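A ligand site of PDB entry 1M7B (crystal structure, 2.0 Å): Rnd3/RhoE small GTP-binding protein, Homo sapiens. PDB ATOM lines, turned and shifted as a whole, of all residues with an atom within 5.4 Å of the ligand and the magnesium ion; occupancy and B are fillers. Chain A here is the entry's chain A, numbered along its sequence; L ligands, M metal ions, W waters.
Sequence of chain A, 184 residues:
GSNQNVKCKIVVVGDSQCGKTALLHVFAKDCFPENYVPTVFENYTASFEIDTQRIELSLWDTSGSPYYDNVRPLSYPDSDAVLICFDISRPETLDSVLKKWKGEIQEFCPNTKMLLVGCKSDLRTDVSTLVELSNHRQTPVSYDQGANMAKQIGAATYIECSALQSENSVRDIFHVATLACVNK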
ATOM      1  N   GLY A  14     -16.118 -18.651  28.532  1.00  0.00           N
ATOM      2  CA  GLY A  14     -15.771 -17.340  28.012  1.00  0.00           C
ATOM      3  C   GLY A  14     -16.138 -16.246  28.997  1.00  0.00           C
ATOM      4  O   GLY A  14     -16.906 -16.494  29.930  1.00  0.00           O
ATOM      5  N   ASP A  15     -15.617 -15.044  28.795  1.00  0.00           N
ATOM      6  CA  ASP A  15     -15.909 -13.927  29.692  1.00  0.00           C
ATOM      7  C   ASP A  15     -17.390 -13.637  29.864  1.00  0.00           C
ATOM      8  O   ASP A  15     -18.214 -13.966  29.002  1.00  0.00           O
ATOM      9  CB  ASP A  15     -15.207 -12.658  29.205  1.00  0.00           C
ATOM     10  CG  ASP A  15     -13.716 -12.674  29.460  1.00  0.00           C
ATOM     11  OD1 ASP A  15     -13.208 -13.712  29.949  1.00  0.00           O
ATOM     12  OD2 ASP A  15     -13.043 -11.663  29.179  1.00  0.00           O
ATOM     13  N   SER A  16     -17.725 -13.017  30.989  1.00  0.00           N
ATOM     14  CA  SER A  16     -19.104 -12.667  31.288  1.00  0.00           C
ATOM     15  C   SER A  16     -19.676 -11.793  30.184  1.00  0.00           C
ATOM     16  O   SER A  16     -18.969 -10.962  29.617  1.00  0.00           O
ATOM     17  CB  SER A  16     -19.181 -11.896  32.613  1.00  0.00           C
ATOM     18  OG  SER A  16     -18.656 -12.675  33.672  1.00  0.00           O
ATOM     19  N   GLN A  17     -20.954 -11.995  29.904  1.00  0.00           N
ATOM     20  CA  GLN A  17     -21.708 -11.260  28.888  1.00  0.00           C
ATOM     21  C   GLN A  17     -21.191 -11.334  27.460  1.00  0.00           C
ATOM     22  O   GLN A  17     -21.538 -10.473  26.642  1.00  0.00           O
ATOM     23  CB  GLN A  17     -21.850  -9.797  29.314  1.00  0.00           C
ATOM     24  CG  GLN A  17     -22.432  -9.630  30.710  1.00  0.00           C
ATOM     25  CD  GLN A  17     -23.078  -8.269  30.931  1.00  0.00           C
ATOM     26  OE1 GLN A  17     -24.179  -8.012  30.445  1.00  0.00           O
ATOM     27  NE2 GLN A  17     -22.399  -7.408  31.659  1.00  0.00           N
ATOM     28  N   CYS A  18     -20.393 -12.347  27.138  1.00  0.00           N
ATOM     29  CA  CYS A  18     -19.900 -12.431  25.764  1.00  0.00           C
ATOM     30  C   CYS A  18     -20.904 -13.102  24.824  1.00  0.00           C
ATOM     31  O   CYS A  18     -20.722 -13.081  23.601  1.00  0.00           O
ATOM     32  CB  CYS A  18     -18.532 -13.130  25.719  1.00  0.00           C
ATOM     33  SG  CYS A  18     -18.520 -14.887  26.112  1.00  0.00           S
ATOM     34  N   GLY A  19     -21.960 -13.688  25.386  1.00  0.00           N
ATOM     35  CA  GLY A  19     -22.990 -14.309  24.570  1.00  0.00           C
ATOM     36  C   GLY A  19     -23.131 -15.825  24.645  1.00  0.00           C
ATOM     37  O   GLY A  19     -23.754 -16.441  23.769  1.00  0.00           O
ATOM     38  N   LYS A  20     -22.562 -16.430  25.679  1.00  0.00           N
ATOM     39  CA  LYS A  20     -22.623 -17.880  25.820  1.00  0.00           C
ATOM     40  C   LYS A  20     -24.051 -18.422  25.961  1.00  0.00           C
ATOM     41  O   LYS A  20     -24.477 -19.325  25.233  1.00  0.00           O
ATOM     42  CB  LYS A  20     -21.786 -18.324  27.021  1.00  0.00           C
ATOM     43  CG  LYS A  20     -20.336 -17.870  26.938  1.00  0.00           C
ATOM     44  CD  LYS A  20     -19.488 -18.387  28.104  1.00  0.00           C
ATOM     45  CE  LYS A  20     -20.004 -17.872  29.440  1.00  0.00           C
ATOM     46  NZ  LYS A  20     -19.909 -16.386  29.557  1.00  0.00           N
ATOM     47  N   THR A  21     -24.800 -17.849  26.896  1.00  0.00           N
ATOM     48  CA  THR A  21     -26.166 -18.292  27.130  1.00  0.00           C
ATOM     49  C   THR A  21     -27.115 -18.077  25.949  1.00  0.00           C
ATOM     50  O   THR A  21     -27.937 -18.940  25.646  1.00  0.00           O
ATOM     51  CB  THR A  21     -26.738 -17.604  28.408  1.00  0.00           C
ATOM     52  OG1 THR A  21     -26.000 -18.077  29.533  1.00  0.00           O
ATOM     53  CG2 THR A  21     -28.211 -17.956  28.611  1.00  0.00           C
ATOM     54  N   ALA A  22     -26.986 -16.933  25.282  1.00  0.00           N
ATOM     55  CA  ALA A  22     -27.839 -16.625  24.138  1.00  0.00           C
ATOM     56  C   ALA A  22     -27.563 -17.631  23.029  1.00  0.00           C
ATOM     57  O   ALA A  22     -28.473 -18.096  22.340  1.00  0.00           O
ATOM     58  CB  ALA A  22     -27.552 -15.225  23.643  1.00  0.00           C
ATOM     59  N   LEU A  23     -26.295 -17.972  22.857  1.00  0.00           N
ATOM     60  CA  LEU A  23     -25.875 -18.922  21.850  1.00  0.00           C
ATOM     61  C   LEU A  23     -26.531 -20.290  22.118  1.00  0.00           C
ATOM     62  O   LEU A  23     -27.094 -20.913  21.220  1.00  0.00           O
ATOM     63  CB  LEU A  23     -24.349 -19.031  21.879  1.00  0.00           C
ATOM     64  CG  LEU A  23     -23.608 -19.975  20.925  1.00  0.00           C
ATOM     65  CD1 LEU A  23     -22.117 -19.628  20.941  1.00  0.00           C
ATOM     66  CD2 LEU A  23     -23.826 -21.406  21.349  1.00  0.00           C
ATOM     67  N   PHE A  32     -34.242 -16.594  21.666  1.00  0.00           N
ATOM     68  CA  PHE A  32     -33.244 -15.658  22.179  1.00  0.00           C
ATOM     69  C   PHE A  32     -33.711 -15.201  23.560  1.00  0.00           C
ATOM     70  O   PHE A  32     -34.873 -14.840  23.734  1.00  0.00           O
ATOM     71  CB  PHE A  32     -33.124 -14.439  21.257  1.00  0.00           C
ATOM     72  CG  PHE A  32     -31.957 -13.538  21.579  1.00  0.00           C
ATOM     73  CD1 PHE A  32     -30.678 -13.852  21.152  1.00  0.00           C
ATOM     74  CD2 PHE A  32     -32.149 -12.375  22.330  1.00  0.00           C
ATOM     75  CE1 PHE A  32     -29.592 -13.026  21.471  1.00  0.00           C
ATOM     76  CE2 PHE A  32     -31.076 -11.545  22.656  1.00  0.00           C
ATOM     77  CZ  PHE A  32     -29.791 -11.878  22.219  1.00  0.00           C
ATOM     78  N   PRO A  33     -32.817 -15.228  24.569  1.00  0.00           N
ATOM     79  CA  PRO A  33     -33.152 -14.817  25.942  1.00  0.00           C
ATOM     80  C   PRO A  33     -33.736 -13.408  25.992  1.00  0.00           C
ATOM     81  O   PRO A  33     -33.166 -12.473  25.422  1.00  0.00           O
ATOM     82  CB  PRO A  33     -31.808 -14.903  26.666  1.00  0.00           C
ATOM     83  CG  PRO A  33     -31.100 -15.991  25.927  1.00  0.00           C
ATOM     84  CD  PRO A  33     -31.408 -15.658  24.490  1.00  0.00           C
ATOM     85  N   TYR A  36     -31.157 -10.568  30.735  1.00  0.00           N
ATOM     86  CA  TYR A  36     -29.841 -11.066  31.103  1.00  0.00           C
ATOM     87  C   TYR A  36     -29.787 -11.526  32.549  1.00  0.00           C
ATOM     88  O   TYR A  36     -30.073 -10.766  33.475  1.00  0.00           O
ATOM     89  CB  TYR A  36     -28.764 -10.010  30.886  1.00  0.00           C
ATOM     90  CG  TYR A  36     -27.423 -10.415  31.480  1.00  0.00           C
ATOM     91  CD1 TYR A  36     -26.710 -11.494  30.975  1.00  0.00           C
ATOM     92  CD2 TYR A  36     -26.908  -9.742  32.586  1.00  0.00           C
ATOM     93  CE1 TYR A  36     -25.520 -11.910  31.556  1.00  0.00           C
ATOM     94  CE2 TYR A  36     -25.702 -10.148  33.178  1.00  0.00           C
ATOM     95  CZ  TYR A  36     -25.027 -11.237  32.652  1.00  0.00           C
ATOM     96  OH  TYR A  36     -23.863 -11.659  33.250  1.00  0.00           O
ATOM     97  N   VAL A  37     -29.403 -12.784  32.738  1.00  0.00           N
ATOM     98  CA  VAL A  37     -29.276 -13.373  34.065  1.00  0.00           C
ATOM     99  C   VAL A  37     -27.926 -14.069  34.092  1.00  0.00           C
ATOM    100  O   VAL A  37     -27.657 -14.934  33.251  1.00  0.00           O
ATOM    101  CB  VAL A  37     -30.386 -14.408  34.332  1.00  0.00           C
ATOM    102  CG1 VAL A  37     -30.168 -15.084  35.674  1.00  0.00           C
ATOM    103  CG2 VAL A  37     -31.752 -13.721  34.294  1.00  0.00           C
ATOM    104  N   PRO A  38     -27.050 -13.694  35.042  1.00  0.00           N
ATOM    105  CA  PRO A  38     -25.731 -14.333  35.121  1.00  0.00           C
ATOM    106  C   PRO A  38     -25.899 -15.843  35.295  1.00  0.00           C
ATOM    107  O   PRO A  38     -26.778 -16.292  36.036  1.00  0.00           O
ATOM    108  CB  PRO A  38     -25.107 -13.677  36.346  1.00  0.00           C
ATOM    109  CG  PRO A  38     -25.726 -12.320  36.359  1.00  0.00           C
ATOM    110  CD  PRO A  38     -27.171 -12.625  36.052  1.00  0.00           C
ATOM    111  N   THR A  39     -25.067 -16.608  34.599  1.00  0.00           N
ATOM    112  CA  THR A  39     -25.146 -18.062  34.680  1.00  0.00           C
ATOM    113  C   THR A  39     -24.125 -18.667  35.630  1.00  0.00           C
ATOM    114  O   THR A  39     -23.025 -18.142  35.766  1.00  0.00           O
ATOM    115  CB  THR A  39     -24.897 -18.704  33.300  1.00  0.00           C
ATOM    116  OG1 THR A  39     -25.740 -18.089  32.322  1.00  0.00           O
ATOM    117  CG2 THR A  39     -25.184 -20.191  33.349  1.00  0.00           C
ATOM    118  N   ASP A  61     -23.621 -24.810  30.003  1.00  0.00           N
ATOM    119  CA  ASP A  61     -23.446 -23.361  30.057  1.00  0.00           C
ATOM    120  C   ASP A  61     -22.715 -23.089  31.376  1.00  0.00           C
ATOM    121  O   ASP A  61     -23.018 -23.720  32.389  1.00  0.00           O
ATOM    122  CB  ASP A  61     -24.819 -22.685  30.074  1.00  0.00           C
ATOM    123  CG  ASP A  61     -24.766 -21.222  29.695  1.00  0.00           C
ATOM    124  OD1 ASP A  61     -23.658 -20.698  29.418  1.00  0.00           O
ATOM    125  OD2 ASP A  61     -25.837 -20.589  29.681  1.00  0.00           O
ATOM    126  N   THR A  62     -21.751 -22.179  31.364  1.00  0.00           N
ATOM    127  CA  THR A  62     -20.977 -21.879  32.578  1.00  0.00           C
ATOM    128  C   THR A  62     -20.901 -20.381  32.884  1.00  0.00           C
ATOM    129  O   THR A  62     -21.401 -19.553  32.121  1.00  0.00           O
ATOM    130  CB  THR A  62     -19.556 -22.417  32.471  1.00  0.00           C
ATOM    131  OG1 THR A  62     -18.883 -21.758  31.392  1.00  0.00           O
ATOM    132  CG2 THR A  62     -19.572 -23.917  32.200  1.00  0.00           C
ATOM    133  N   SER A  63     -20.255 -20.054  34.001  1.00  0.00           N
ATOM    134  CA  SER A  63     -20.092 -18.658  34.413  1.00  0.00           C
ATOM    135  C   SER A  63     -18.791 -18.077  33.895  1.00  0.00           C
ATOM    136  O   SER A  63     -17.745 -18.709  33.971  1.00  0.00           O
ATOM    137  CB  SER A  63     -20.105 -18.541  35.954  1.00  0.00           C
ATOM    138  OG  SER A  63     -19.655 -17.262  36.376  1.00  0.00           O
ATOM    139  N   GLY A  64     -18.847 -16.856  33.381  1.00  0.00           N
ATOM    140  CA  GLY A  64     -17.634 -16.228  32.905  1.00  0.00           C
ATOM    141  C   GLY A  64     -16.963 -15.459  34.035  1.00  0.00           C
ATOM    142  O   GLY A  64     -15.890 -14.875  33.860  1.00  0.00           O
ATOM    143  N   SER A  65     -17.588 -15.480  35.205  1.00  0.00           N
ATOM    144  CA  SER A  65     -17.067 -14.749  36.353  1.00  0.00           C
ATOM    145  C   SER A  65     -15.946 -15.412  37.137  1.00  0.00           C
ATOM    146  O   SER A  65     -15.947 -16.622  37.370  1.00  0.00           O
ATOM    147  CB  SER A  65     -18.200 -14.426  37.337  1.00  0.00           C
ATOM    148  OG  SER A  65     -17.663 -13.881  38.536  1.00  0.00           O
ATOM    149  N   CYS A 119     -18.560 -14.217  19.167  1.00  0.00           N
ATOM    150  CA  CYS A 119     -19.990 -13.976  19.322  1.00  0.00           C
ATOM    151  C   CYS A 119     -20.365 -12.525  19.064  1.00  0.00           C
ATOM    152  O   CYS A 119     -19.517 -11.630  19.150  1.00  0.00           O
ATOM    153  CB  CYS A 119     -20.451 -14.364  20.728  1.00  0.00           C
ATOM    154  SG  CYS A 119     -20.240 -16.103  21.126  1.00  0.00           S
ATOM    155  N   LYS A 120     -21.648 -12.304  18.796  1.00  0.00           N
ATOM    156  CA  LYS A 120     -22.198 -10.974  18.521  1.00  0.00           C
ATOM    157  C   LYS A 120     -21.562 -10.362  17.261  1.00  0.00           C
ATOM    158  O   LYS A 120     -21.159  -9.204  17.275  1.00  0.00           O
ATOM    159  CB  LYS A 120     -21.986 -10.039  19.710  1.00  0.00           C
ATOM    160  CG  LYS A 120     -22.464 -10.575  21.069  1.00  0.00           C
ATOM    161  CD  LYS A 120     -22.425  -9.470  22.127  1.00  0.00           C
ATOM    162  CE  LYS A 120     -22.585 -10.017  23.558  1.00  0.00           C
ATOM    163  NZ  LYS A 120     -22.503  -8.901  24.551  1.00  0.00           N
ATOM    164  N   SER A 121     -21.492 -11.121  16.178  1.00  0.00           N
ATOM    165  CA  SER A 121     -20.883 -10.591  14.956  1.00  0.00           C
ATOM    166  C   SER A 121     -21.703  -9.422  14.420  1.00  0.00           C
ATOM    167  O   SER A 121     -21.156  -8.549  13.747  1.00  0.00           O
ATOM    168  CB  SER A 121     -20.757 -11.672  13.887  1.00  0.00           C
ATOM    169  OG  SER A 121     -22.018 -12.147  13.487  1.00  0.00           O
ATOM    170  N   ASP A 122     -22.997  -9.390  14.737  1.00  0.00           N
ATOM    171  CA  ASP A 122     -23.854  -8.314  14.273  1.00  0.00           C
ATOM    172  C   ASP A 122     -23.390  -6.937  14.746  1.00  0.00           C
ATOM    173  O   ASP A 122     -23.706  -5.926  14.122  1.00  0.00           O
ATOM    174  CB  ASP A 122     -25.308  -8.532  14.730  1.00  0.00           C
ATOM    175  CG  ASP A 122     -25.447  -8.637  16.262  1.00  0.00           C
ATOM    176  OD1 ASP A 122     -25.086  -9.693  16.809  1.00  0.00           O
ATOM    177  OD2 ASP A 122     -25.915  -7.669  16.897  1.00  0.00           O
ATOM    178  N   LEU A 123     -22.628  -6.892  15.841  1.00  0.00           N
ATOM    179  CA  LEU A 123     -22.171  -5.609  16.367  1.00  0.00           C
ATOM    180  C   LEU A 123     -20.965  -5.026  15.642  1.00  0.00           C
ATOM    181  O   LEU A 123     -20.647  -3.845  15.811  1.00  0.00           O
ATOM    182  CB  LEU A 123     -21.865  -5.737  17.860  1.00  0.00           C
ATOM    183  CG  LEU A 123     -23.067  -6.067  18.768  1.00  0.00           C
ATOM    184  CD1 LEU A 123     -22.633  -6.074  20.235  1.00  0.00           C
ATOM    185  CD2 LEU A 123     -24.161  -5.029  18.543  1.00  0.00           C
ATOM    186  N   CYS A 161     -20.465 -15.987  14.897  1.00  0.00           N
ATOM    187  CA  CYS A 161     -21.915 -16.127  14.863  1.00  0.00           C
ATOM    188  C   CYS A 161     -22.612 -14.920  15.468  1.00  0.00           C
ATOM    189  O   CYS A 161     -21.975 -14.043  16.049  1.00  0.00           O
ATOM    190  CB  CYS A 161     -22.357 -17.384  15.608  1.00  0.00           C
ATOM    191  SG  CYS A 161     -22.087 -17.335  17.401  1.00  0.00           S
ATOM    192  N   SER A 162     -23.924 -14.873  15.299  1.00  0.00           N
ATOM    193  CA  SER A 162     -24.754 -13.830  15.884  1.00  0.00           C
ATOM    194  C   SER A 162     -26.043 -14.502  16.335  1.00  0.00           C
ATOM    195  O   SER A 162     -26.949 -14.749  15.537  1.00  0.00           O
ATOM    196  CB  SER A 162     -25.080 -12.739  14.861  1.00  0.00           C
ATOM    197  OG  SER A 162     -26.021 -11.835  15.419  1.00  0.00           O
ATOM    198  N   ALA A 163     -26.113 -14.830  17.618  1.00  0.00           N
ATOM    199  CA  ALA A 163     -27.288 -15.477  18.160  1.00  0.00           C
ATOM    200  C   ALA A 163     -28.503 -14.571  17.996  1.00  0.00           C
ATOM    201  O   ALA A 163     -29.635 -15.042  17.925  1.00  0.00           O
ATOM    202  CB  ALA A 163     -27.075 -15.793  19.640  1.00  0.00           C
ATOM    203  N   LEU A 164     -28.263 -13.269  17.941  1.00  0.00           N
ATOM    204  CA  LEU A 164     -29.349 -12.297  17.813  1.00  0.00           C
ATOM    205  C   LEU A 164     -29.942 -12.221  16.413  1.00  0.00           C
ATOM    206  O   LEU A 164     -31.165 -12.215  16.261  1.00  0.00           O
ATOM    207  CB  LEU A 164     -28.855 -10.906  18.227  1.00  0.00           C
ATOM    208  CG  LEU A 164     -29.829  -9.858  18.803  1.00  0.00           C
ATOM    209  CD1 LEU A 164     -29.457  -8.503  18.244  1.00  0.00           C
ATOM    210  CD2 LEU A 164     -31.277 -10.184  18.455  1.00  0.00           C
ATOM    211  N   GLN A 165     -29.092 -12.159  15.394  1.00  0.00           N
ATOM    212  CA  GLN A 165     -29.568 -12.024  14.028  1.00  0.00           C
ATOM    213  C   GLN A 165     -29.597 -13.250  13.129  1.00  0.00           C
ATOM    214  O   GLN A 165     -30.361 -13.290  12.165  1.00  0.00           O
ATOM    215  CB  GLN A 165     -28.767 -10.914  13.318  1.00  0.00           C
ATOM    216  CG  GLN A 165     -28.966  -9.536  13.945  1.00  0.00           C
ATOM    217  CD  GLN A 165     -28.428  -8.407  13.090  1.00  0.00           C
ATOM    218  OE1 GLN A 165     -28.566  -7.230  13.444  1.00  0.00           O
ATOM    219  NE2 GLN A 165     -27.804  -8.738  11.964  1.00  0.00           N
HETATM  220  P1  LIG L   1     -22.439 -14.896  31.912  1.00  0.00           P
HETATM  221  O1  LIG L   1     -22.361 -13.701  32.825  1.00  0.00           O
HETATM  222  O2  LIG L   1     -23.507 -15.880  32.260  1.00  0.00           O
HETATM  223  O3  LIG L   1     -21.109 -15.492  31.804  1.00  0.00           O
HETATM  224  O4  LIG L   1     -22.837 -14.150  30.338  1.00  0.00           O
HETATM  225  P2  LIG L   1     -23.099 -14.803  28.830  1.00  0.00           P
HETATM  226  O5  LIG L   1     -21.754 -14.993  28.138  1.00  0.00           O
HETATM  227  O6  LIG L   1     -23.854 -16.024  28.964  1.00  0.00           O
HETATM  228  O7  LIG L   1     -23.946 -13.723  28.106  1.00  0.00           O
HETATM  229  P3  LIG L   1     -25.443 -13.725  27.498  1.00  0.00           P
HETATM  230  O8  LIG L   1     -25.674 -14.744  26.501  1.00  0.00           O
HETATM  231  O9  LIG L   1     -26.371 -13.755  28.725  1.00  0.00           O
HETATM  232  O10 LIG L   1     -25.451 -12.247  26.708  1.00  0.00           O
HETATM  233  C1  LIG L   1     -25.193 -11.108  27.646  1.00  0.00           C
HETATM  234  C2  LIG L   1     -25.879  -9.922  26.795  1.00  0.00           C
HETATM  235  O11 LIG L   1     -25.460  -9.837  25.409  1.00  0.00           O
HETATM  236  C3  LIG L   1     -27.338  -9.915  26.775  1.00  0.00           C
HETATM  237  O12 LIG L   1     -27.863  -8.665  27.155  1.00  0.00           O
HETATM  238  C4  LIG L   1     -27.837 -10.387  25.377  1.00  0.00           C
HETATM  239  O13 LIG L   1     -29.009  -9.893  25.018  1.00  0.00           O
HETATM  240  C5  LIG L   1     -26.545  -9.774  24.472  1.00  0.00           C
HETATM  241  N1  LIG L   1     -26.259 -10.707  23.314  1.00  0.00           N
HETATM  242  C6  LIG L   1     -26.123 -12.091  23.448  1.00  0.00           C
HETATM  243  N2  LIG L   1     -25.888 -12.407  22.148  1.00  0.00           N
HETATM  244  C7  LIG L   1     -25.879 -11.323  21.258  1.00  0.00           C
HETATM  245  C8  LIG L   1     -25.690 -11.328  20.001  1.00  0.00           C
HETATM  246  O14 LIG L   1     -25.453 -12.155  19.062  1.00  0.00           O
HETATM  247  N3  LIG L   1     -25.758  -9.904  19.418  1.00  0.00           N
HETATM  248  C9  LIG L   1     -25.990  -8.959  20.287  1.00  0.00           C
HETATM  249  N4  LIG L   1     -26.058  -7.584  19.716  1.00  0.00           N
HETATM  250  N5  LIG L   1     -26.200  -8.965  21.619  1.00  0.00           N
HETATM  251  C10 LIG L   1     -26.115 -10.261  22.027  1.00  0.00           C
HETATM  252 MG    MG M   1     -24.677 -16.891  30.731  1.00  0.00          MG
HETATM  253  O   HOH W   1     -20.841 -13.599  35.004  1.00  0.00           O
HETATM  254  O   HOH W   2     -28.971 -13.710  28.243  1.00  0.00           O
HETATM  255  O   HOH W   3     -30.563 -11.700  26.325  1.00  0.00           O
HETATM  256  O   HOH W   4     -26.256 -15.431  30.861  1.00  0.00           O
HETATM  257  O   HOH W   5     -24.236 -14.859  21.571  1.00  0.00           O
HETATM  258  O   HOH W   6     -23.199 -18.411  30.569  1.00  0.00           O
HETATM  259  O   HOH W   7     -23.459 -14.631  18.978  1.00  0.00           O
HETATM  260  O   HOH W   8     -26.421  -5.172  21.412  1.00  0.00           O
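The backbone NH of Thr 21 is in hydrogen-bond range of an oxygen (O8) of the ligand, 3.2 Å away. N of Thr 39 sits close to O2 of the ligand (2.9 Å). An oxygen (O1) of the ligand sits at hydrogen-bond distance from the side-chain hydroxyl of Tyr 36 (2.6 Å). N of Lys 20 sits at hydrogen-bond distance from O5 of the ligand (3.0 Å). The side-chain amino group (NZ) of Lys 20 lies within salt-bridge range of an oxygen (O3) of the ligand (2.7 Å). A nitrogen (N3) of the ligand lies within hydrogen-bond range of the side-chain carboxylate (OD1) of Asp 122, 2.7 Å away. The backbone NH of Ala 22 sits at hydrogen-bond distance from an oxygen (O8) of the ligand. N of Gln 17 is in hydrogen-bond range of O4 of the ligand. The backbone NH (N) of Gly 19 lies within hydrogen-bond range of an oxygen (O5) of the ligand (3.1 Å). The backbone NH (N) of Gly 64 lies within hydrogen-bond range of an oxygen (O3) of the ligand, at 3.1 Å. An oxygen (O14) of the ligand is in hydrogen-bond range of the backbone NH of Ala 163, 3.1 Å away. The backbone NH of Cys 18 is in hydrogen-bond range of an oxygen (O5) of the ligand (3.1 Å). An oxygen (O11) of the ligand sits at hydrogen-bond distance from the side-chain amino group (NZ) of Lys 120. N of Leu 164 sits at hydrogen-bond distance from O14 of the ligand, at 3.2 Å.
The magnesium ion is bound by water W6, 2.1 Å away. The magnesium ion is bound by an oxygen (O6) of the ligand. The magnesium ion is bound by the side-chain hydroxyl (OG1) of Thr 21 (2.1 Å). The magnesium ion is bound by water W4 (2.2 Å). O2 of the ligand is bound to the magnesium ion, at 2.2 Å. OG1 of Thr 39 binds the magnesium ion (2.3 Å).
OG1 of Thr 21 lies close to OD2 of Asp 61. The side-chain amino group (NZ) of Lys 20 lies within hydrogen-bond range of the backbone carbonyl oxygen (O) of Asp 15 (3.0 Å). The side-chain amino group (NZ) of Lys 20 lies within hydrogen-bond range of the backbone carbonyl oxygen (O) of Gly 14 (3.0 Å). The side-chain amino group (NZ) of Lys 120 sits at hydrogen-bond distance from the backbone carbonyl oxygen (O) of Gln 17 (2.8 Å). The side-chain sulfur (SG) of Cys 18 lies within hydrogen-bond range of the backbone carbonyl oxygen (O) of Asp 15, at 3.0 Å. The backbone NH of Lys 120 sits at hydrogen-bond distance from the backbone carbonyl oxygen of Cys 161, 3.3 Å away. OG of Ser 16 is in hydrogen-bond range of N of Ser 65 (3.4 Å). The side-chain hydroxyl (OG) of Ser 162 sits at hydrogen-bond distance from the backbone NH (N) of Gln 165, 3.1 Å away.
Asp 15 touches the ligand. Ser 16 touches the ligand (CA to O3, 3.5 Å). CZ of Phe 32 touches O13 of the ligand, 3.5 Å away. Pro 38 touches the ligand. Leu 123 touches the ligand (CD2 to N4, 3.4 Å). Ser 162 touches the ligand. Within 4 Å of the ligand: Asp 15, Ser 16, Gln 17, Cys 18, Gly 19, Lys 20, Thr 21, Ala 22, Phe 32, Tyr 36, Pro 38, Thr 39, Gly 64, Lys 120, Asp 122, Leu 123, Ser 162, Ala 163 and Leu 164.
Water W6 bridges OD1 of Asp 61 (2.6 Å) and O of Thr 62 (2.6 Å). Water W4 lies within hydrogen-bond range of an oxygen (O9) of the ligand (2.7 Å) and the backbone carbonyl oxygen of Val 37 (2.8 Å). Water W1 bridges an oxygen (O1) of the ligand (2.7 Å) and the side-chain hydroxyl of Ser 16 (2.7 Å). Water W3 bridges O13 of the ligand (2.7 Å) and O of Pro 33 (2.9 Å). Water W5 lies within hydrogen-bond range of the backbone carbonyl oxygen of Gly 19 and a nitrogen (N2) of the ligand. Water W7 lies within hydrogen-bond range of the backbone NH (N) of Lys 120 (3.0 Å), the backbone NH (N) of Ala 163 (3.0 Å), an oxygen (O14) of the ligand (3.2 Å) and the backbone carbonyl oxygen (O) of Cys 161 (3.3 Å).
Of the 31 residues printed, 2 come within 4 Å of the magnesium ion.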
